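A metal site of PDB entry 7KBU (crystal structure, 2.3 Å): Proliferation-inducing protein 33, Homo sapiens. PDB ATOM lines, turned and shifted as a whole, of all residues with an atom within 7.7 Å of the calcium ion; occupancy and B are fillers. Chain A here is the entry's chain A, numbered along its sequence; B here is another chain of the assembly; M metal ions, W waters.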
ATOM      1  N   PRO A  83       4.445   9.983  26.041  1.00  0.00           N
ATOM      2  CA  PRO A  83       5.498   8.994  26.268  1.00  0.00           C
ATOM      3  C   PRO A  83       6.173   8.538  24.980  1.00  0.00           C
ATOM      4  O   PRO A  83       5.700   8.716  23.857  1.00  0.00           O
ATOM      5  CB  PRO A  83       4.754   7.821  26.918  1.00  0.00           C
ATOM      6  CG  PRO A  83       3.353   7.974  26.521  1.00  0.00           C
ATOM      7  CD  PRO A  83       3.096   9.434  26.257  1.00  0.00           C
ATOM      8  N   THR A  84       7.310   7.890  25.214  1.00  0.00           N
ATOM      9  CA  THR A  84       8.133   7.324  24.161  1.00  0.00           C
ATOM     10  C   THR A  84       7.469   6.110  23.557  1.00  0.00           C
ATOM     11  O   THR A  84       6.980   5.254  24.278  1.00  0.00           O
ATOM     12  CB  THR A  84       9.487   6.926  24.743  1.00  0.00           C
ATOM     13  OG1 THR A  84      10.112   8.107  25.240  1.00  0.00           O
ATOM     14  CG2 THR A  84      10.380   6.252  23.698  1.00  0.00           C
ATOM     15  N   CYS A  85       7.430   6.037  22.230  1.00  0.00           N
ATOM     16  CA  CYS A  85       6.842   4.881  21.596  1.00  0.00           C
ATOM     17  C   CYS A  85       7.592   3.625  22.021  1.00  0.00           C
ATOM     18  O   CYS A  85       8.814   3.656  22.184  1.00  0.00           O
ATOM     19  CB  CYS A  85       6.901   4.996  20.064  1.00  0.00           C
ATOM     20  SG  CYS A  85       5.894   6.307  19.345  1.00  0.00           S
ATOM     21  N   THR A  86       6.853   2.530  22.208  1.00  0.00           N
ATOM     22  CA  THR A  86       7.432   1.208  22.359  1.00  0.00           C
ATOM     23  C   THR A  86       7.617   0.590  20.985  1.00  0.00           C
ATOM     24  O   THR A  86       7.059   1.058  19.975  1.00  0.00           O
ATOM     25  CB  THR A  86       6.528   0.298  23.201  1.00  0.00           C
ATOM     26  OG1 THR A  86       5.358  -0.054  22.424  1.00  0.00           O
ATOM     27  CG2 THR A  86       6.103   0.981  24.507  1.00  0.00           C
ATOM     28  N   PHE A  88       6.448  -2.178  19.801  1.00  0.00           N
ATOM     29  CA  PHE A  88       5.204  -2.713  19.228  1.00  0.00           C
ATOM     30  C   PHE A  88       4.232  -1.614  18.835  1.00  0.00           C
ATOM     31  O   PHE A  88       3.400  -1.837  17.947  1.00  0.00           O
ATOM     32  CB  PHE A  88       4.536  -3.712  20.182  1.00  0.00           C
ATOM     33  CG  PHE A  88       4.319  -3.183  21.564  1.00  0.00           C
ATOM     34  CD1 PHE A  88       5.303  -3.322  22.543  1.00  0.00           C
ATOM     35  CD2 PHE A  88       3.137  -2.518  21.891  1.00  0.00           C
ATOM     36  CE1 PHE A  88       5.111  -2.808  23.824  1.00  0.00           C
ATOM     37  CE2 PHE A  88       2.933  -2.008  23.167  1.00  0.00           C
ATOM     38  CZ  PHE A  88       3.928  -2.147  24.138  1.00  0.00           C
ATOM     39  N   GLU A  89       4.342  -0.399  19.416  1.00  0.00           N
ATOM     40  CA  GLU A  89       3.590   0.738  18.881  1.00  0.00           C
ATOM     41  C   GLU A  89       4.127   1.117  17.498  1.00  0.00           C
ATOM     42  O   GLU A  89       3.377   1.661  16.668  1.00  0.00           O
ATOM     43  CB  GLU A  89       3.653   1.931  19.836  1.00  0.00           C
ATOM     44  CG  GLU A  89       2.725   1.850  21.092  1.00  0.00           C
ATOM     45  CD  GLU A  89       2.905   3.041  22.094  1.00  0.00           C
ATOM     46  OE1 GLU A  89       4.016   3.224  22.652  1.00  0.00           O
ATOM     47  OE2 GLU A  89       1.935   3.786  22.340  1.00  0.00           O
ATOM     48  N   LEU A 190       3.449   8.527  13.861  1.00  0.00           N
ATOM     49  CA  LEU A 190       3.051   7.770  15.051  1.00  0.00           C
ATOM     50  C   LEU A 190       2.354   8.628  16.124  1.00  0.00           C
ATOM     51  O   LEU A 190       1.586   8.065  16.923  1.00  0.00           O
ATOM     52  CB  LEU A 190       4.257   7.061  15.643  1.00  0.00           C
ATOM     53  CG  LEU A 190       4.720   5.945  14.679  1.00  0.00           C
ATOM     54  CD1 LEU A 190       5.984   5.261  15.141  1.00  0.00           C
ATOM     55  CD2 LEU A 190       3.642   4.901  14.489  1.00  0.00           C
ATOM     56  N   VAL A 191       2.551   9.939  16.173  1.00  0.00           N
ATOM     57  CA  VAL A 191       1.839  10.746  17.151  1.00  0.00           C
ATOM     58  C   VAL A 191       0.319  10.644  16.967  1.00  0.00           C
ATOM     59  O   VAL A 191      -0.386  10.291  17.912  1.00  0.00           O
ATOM     60  CB  VAL A 191       2.335  12.205  17.129  1.00  0.00           C
ATOM     61  CG1 VAL A 191       1.533  13.030  18.099  1.00  0.00           C
ATOM     62  CG2 VAL A 191       3.826  12.266  17.535  1.00  0.00           C
ATOM     63  N   MET A 193      -1.334   8.305  15.324  1.00  0.00           N
ATOM     64  CA  MET A 193      -1.794   6.919  15.321  1.00  0.00           C
ATOM     65  C   MET A 193      -1.698   6.256  16.692  1.00  0.00           C
ATOM     66  O   MET A 193      -2.549   5.456  17.066  1.00  0.00           O
ATOM     67  CB  MET A 193      -0.956   6.097  14.341  1.00  0.00           C
ATOM     68  CG  MET A 193      -1.134   6.401  12.865  1.00  0.00           C
ATOM     69  SD  MET A 193      -0.179   5.201  11.924  1.00  0.00           S
ATOM     70  CE  MET A 193      -1.183   3.709  12.206  1.00  0.00           C
ATOM     71  N   GLU A 194      -0.670   6.611  17.461  1.00  0.00           N
ATOM     72  CA  GLU A 194      -0.309   5.886  18.659  1.00  0.00           C
ATOM     73  C   GLU A 194      -0.124   6.802  19.859  1.00  0.00           C
ATOM     74  O   GLU A 194       0.097   6.324  20.965  1.00  0.00           O
ATOM     75  CB  GLU A 194       0.997   5.096  18.394  1.00  0.00           C
ATOM     76  CG  GLU A 194       0.897   3.635  17.764  1.00  0.00           C
ATOM     77  CD  GLU A 194      -0.105   2.721  18.449  1.00  0.00           C
ATOM     78  OE1 GLU A 194      -0.571   1.774  17.809  1.00  0.00           O
ATOM     79  OE2 GLU A 194      -0.468   2.972  19.630  1.00  0.00           O
ATOM     80  N   HIS A 195      -0.173   8.132  19.670  1.00  0.00           N
ATOM     81  CA  HIS A 195      -0.075   9.077  20.776  1.00  0.00           C
ATOM     82  C   HIS A 195       1.238   8.907  21.525  1.00  0.00           C
ATOM     83  O   HIS A 195       1.290   8.986  22.745  1.00  0.00           O
ATOM     84  CB  HIS A 195      -1.253   8.899  21.720  1.00  0.00           C
ATOM     85  CG  HIS A 195      -1.545  10.095  22.567  1.00  0.00           C
ATOM     86  ND1 HIS A 195      -1.408  11.383  22.099  1.00  0.00           N
ATOM     87  CD2 HIS A 195      -1.991  10.190  23.846  1.00  0.00           C
ATOM     88  CE1 HIS A 195      -1.724  12.226  23.067  1.00  0.00           C
ATOM     89  NE2 HIS A 195      -2.072  11.527  24.139  1.00  0.00           N
ATOM     90  N   CYS A 196       2.309   8.646  20.785  1.00  0.00           N
ATOM     91  CA  CYS A 196       3.624   8.490  21.359  1.00  0.00           C
ATOM     92  C   CYS A 196       4.651   9.130  20.447  1.00  0.00           C
ATOM     93  O   CYS A 196       4.420   9.334  19.251  1.00  0.00           O
ATOM     94  CB  CYS A 196       3.973   7.007  21.595  1.00  0.00           C
ATOM     95  SG  CYS A 196       4.030   6.047  20.099  1.00  0.00           S
ATOM     96  N   ILE A 197       5.794   9.455  21.033  1.00  0.00           N
ATOM     97  CA  ILE A 197       6.899  10.088  20.312  1.00  0.00           C
ATOM     98  C   ILE A 197       8.039   9.080  20.229  1.00  0.00           C
ATOM     99  O   ILE A 197       8.483   8.538  21.239  1.00  0.00           O
ATOM    100  CB  ILE A 197       7.337  11.387  21.020  1.00  0.00           C
ATOM    101  CG1 ILE A 197       8.309  12.177  20.146  1.00  0.00           C
ATOM    102  CG2 ILE A 197       7.966  11.075  22.393  1.00  0.00           C
ATOM    103  CD1 ILE A 197       7.587  12.961  19.067  1.00  0.00           C
ATOM    104  N   PRO B  83      -0.695   9.845  29.747  1.00  0.00           N
ATOM    105  CA  PRO B  83      -1.783  10.679  29.236  1.00  0.00           C
ATOM    106  C   PRO B  83      -3.076   9.885  29.044  1.00  0.00           C
ATOM    107  O   PRO B  83      -3.103   8.657  29.027  1.00  0.00           O
ATOM    108  CB  PRO B  83      -1.248  11.153  27.883  1.00  0.00           C
ATOM    109  CG  PRO B  83      -0.389  10.040  27.440  1.00  0.00           C
ATOM    110  CD  PRO B  83       0.285   9.541  28.699  1.00  0.00           C
ATOM    111  N   CYS B  85      -6.085   8.235  27.107  1.00  0.00           N
ATOM    112  CA  CYS B  85      -6.160   7.536  25.833  1.00  0.00           C
ATOM    113  C   CYS B  85      -6.943   8.343  24.801  1.00  0.00           C
ATOM    114  O   CYS B  85      -7.964   8.952  25.131  1.00  0.00           O
ATOM    115  CB  CYS B  85      -6.829   6.161  25.985  1.00  0.00           C
ATOM    116  SG  CYS B  85      -6.002   4.945  27.077  1.00  0.00           S
ATOM    117  N   THR B  86      -6.472   8.329  23.555  1.00  0.00           N
ATOM    118  CA  THR B  86      -7.177   8.851  22.387  1.00  0.00           C
ATOM    119  C   THR B  86      -7.987   7.752  21.687  1.00  0.00           C
ATOM    120  O   THR B  86      -7.794   6.547  21.918  1.00  0.00           O
ATOM    121  CB  THR B  86      -6.181   9.458  21.406  1.00  0.00           C
ATOM    122  OG1 THR B  86      -5.394   8.402  20.830  1.00  0.00           O
ATOM    123  CG2 THR B  86      -5.262  10.436  22.109  1.00  0.00           C
ATOM    124  N   PHE B  88      -7.833   6.543  18.646  1.00  0.00           N
ATOM    125  CA  PHE B  88      -7.104   5.558  17.879  1.00  0.00           C
ATOM    126  C   PHE B  88      -6.285   4.634  18.767  1.00  0.00           C
ATOM    127  O   PHE B  88      -5.888   3.556  18.323  1.00  0.00           O
ATOM    128  CB  PHE B  88      -6.202   6.241  16.857  1.00  0.00           C
ATOM    129  CG  PHE B  88      -6.934   6.742  15.637  1.00  0.00           C
ATOM    130  CD1 PHE B  88      -8.309   6.580  15.495  1.00  0.00           C
ATOM    131  CD2 PHE B  88      -6.234   7.376  14.634  1.00  0.00           C
ATOM    132  CE1 PHE B  88      -8.972   7.056  14.355  1.00  0.00           C
ATOM    133  CE2 PHE B  88      -6.891   7.844  13.503  1.00  0.00           C
ATOM    134  CZ  PHE B  88      -8.262   7.690  13.365  1.00  0.00           C
ATOM    135  N   GLU B  89      -6.017   5.010  20.015  1.00  0.00           N
ATOM    136  CA  GLU B  89      -5.349   4.073  20.908  1.00  0.00           C
ATOM    137  C   GLU B  89      -6.283   2.979  21.387  1.00  0.00           C
ATOM    138  O   GLU B  89      -5.869   1.824  21.538  1.00  0.00           O
ATOM    139  CB  GLU B  89      -4.757   4.816  22.111  1.00  0.00           C
ATOM    140  CG  GLU B  89      -3.594   5.720  21.777  1.00  0.00           C
ATOM    141  CD  GLU B  89      -3.061   6.436  23.007  1.00  0.00           C
ATOM    142  OE1 GLU B  89      -3.760   7.354  23.481  1.00  0.00           O
ATOM    143  OE2 GLU B  89      -1.954   6.083  23.498  1.00  0.00           O
ATOM    144  N   LEU B 190      -5.231  -1.341  28.740  1.00  0.00           N
ATOM    145  CA  LEU B 190      -4.651  -0.322  27.881  1.00  0.00           C
ATOM    146  C   LEU B 190      -3.424   0.345  28.473  1.00  0.00           C
ATOM    147  O   LEU B 190      -2.616   0.886  27.723  1.00  0.00           O
ATOM    148  CB  LEU B 190      -5.725   0.719  27.556  1.00  0.00           C
ATOM    149  CG  LEU B 190      -6.758   0.169  26.575  1.00  0.00           C
ATOM    150  CD1 LEU B 190      -7.906   1.121  26.461  1.00  0.00           C
ATOM    151  CD2 LEU B 190      -6.117  -0.071  25.213  1.00  0.00           C
ATOM    152  N   VAL B 191      -3.253   0.320  29.786  1.00  0.00           N
ATOM    153  CA  VAL B 191      -2.038   0.913  30.365  1.00  0.00           C
ATOM    154  C   VAL B 191      -0.790   0.222  29.819  1.00  0.00           C
ATOM    155  O   VAL B 191       0.094   0.891  29.262  1.00  0.00           O
ATOM    156  CB  VAL B 191      -2.086   0.868  31.897  1.00  0.00           C
ATOM    157  CG1 VAL B 191      -0.723   1.286  32.501  1.00  0.00           C
ATOM    158  CG2 VAL B 191      -3.180   1.775  32.381  1.00  0.00           C
ATOM    159  N   MET B 193      -0.653  -1.936  27.228  1.00  0.00           N
ATOM    160  CA  MET B 193      -0.675  -2.092  25.779  1.00  0.00           C
ATOM    161  C   MET B 193      -0.521  -0.776  25.033  1.00  0.00           C
ATOM    162  O   MET B 193       0.024  -0.769  23.932  1.00  0.00           O
ATOM    163  CB  MET B 193      -1.950  -2.784  25.331  1.00  0.00           C
ATOM    164  CG  MET B 193      -2.008  -4.234  25.809  1.00  0.00           C
ATOM    165  SD  MET B 193      -3.467  -5.107  25.213  1.00  0.00           S
ATOM    166  CE  MET B 193      -3.327  -4.921  23.431  1.00  0.00           C
ATOM    167  N   GLU B 194      -0.978   0.342  25.602  1.00  0.00           N
ATOM    168  CA  GLU B 194      -0.983   1.610  24.888  1.00  0.00           C
ATOM    169  C   GLU B 194      -0.361   2.751  25.674  1.00  0.00           C
ATOM    170  O   GLU B 194      -0.171   3.828  25.106  1.00  0.00           O
ATOM    171  CB  GLU B 194      -2.411   2.008  24.489  1.00  0.00           C
ATOM    172  CG  GLU B 194      -2.837   1.362  23.187  1.00  0.00           C
ATOM    173  CD  GLU B 194      -2.002   1.838  21.973  1.00  0.00           C
ATOM    174  OE1 GLU B 194      -1.340   2.939  22.027  1.00  0.00           O
ATOM    175  OE2 GLU B 194      -2.012   1.100  20.974  1.00  0.00           O
ATOM    176  N   HIS B 195       0.003   2.537  26.940  1.00  0.00           N
ATOM    177  CA  HIS B 195       0.650   3.571  27.744  1.00  0.00           C
ATOM    178  C   HIS B 195      -0.242   4.802  27.854  1.00  0.00           C
ATOM    179  O   HIS B 195       0.216   5.938  27.781  1.00  0.00           O
ATOM    180  CB  HIS B 195       2.039   3.922  27.179  1.00  0.00           C
ATOM    181  CG  HIS B 195       3.059   2.827  27.338  1.00  0.00           C
ATOM    182  ND1 HIS B 195       4.408   3.071  27.463  1.00  0.00           N
ATOM    183  CD2 HIS B 195       2.911   1.475  27.389  1.00  0.00           C
ATOM    184  CE1 HIS B 195       5.059   1.918  27.586  1.00  0.00           C
ATOM    185  NE2 HIS B 195       4.174   0.938  27.551  1.00  0.00           N
ATOM    186  N   CYS B 196      -1.541   4.562  28.029  1.00  0.00           N
ATOM    187  CA  CYS B 196      -2.506   5.633  28.217  1.00  0.00           C
ATOM    188  C   CYS B 196      -3.541   5.186  29.246  1.00  0.00           C
ATOM    189  O   CYS B 196      -3.713   3.989  29.494  1.00  0.00           O
ATOM    190  CB  CYS B 196      -3.162   5.991  26.890  1.00  0.00           C
ATOM    191  SG  CYS B 196      -4.194   4.670  26.228  1.00  0.00           S
HETATM  192 CA    CA M   1      -0.045   4.858  22.908  1.00  0.00          CA
HETATM  193  O   HOH W   1       1.380   6.251  24.098  1.00  0.00           O
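Of the 24 residues printed, 4 come within 4 Å of the calcium ion. The nearest printed residue that does not touch the calcium ion is His 195 of chain A (4.3 Å).
OE1 of Glu 89 of chain A sits at hydrogen-bond distance from N of Thr 86 of chain A, at 3.0 Å. The side-chain sulfur of Cys 196 of chain A is disulfide-bonded to the side-chain sulfur of Cys 85 of chain A, 2.0 Å away. OE1 of Glu 89 of chain B sits at hydrogen-bond distance from N of Thr 86 of chain B (2.9 Å). The side-chain sulfur (SG) of Cys 85 of chain B is disulfide-bonded to the side-chain sulfur (SG) of Cys 196 of chain B, at 2.0 Å.
The calcium ion is bound by water W1 (2.3 Å), the side-chain carboxylate (OE2) of Glu 89 of chain A (2.3 Å), the side-chain carboxylate (OE2) of Glu 89 of chain B (2.3 Å), the backbone carbonyl oxygen (O) of Glu 194 of chain B (2.4 Å), the backbone carbonyl oxygen (O) of Glu 194 of chain A (2.4 Å) and the side-chain carboxylate (OE1) of Glu 194 of chain B (2.5 Å). The calcium ion has six donor atoms within binding distance.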
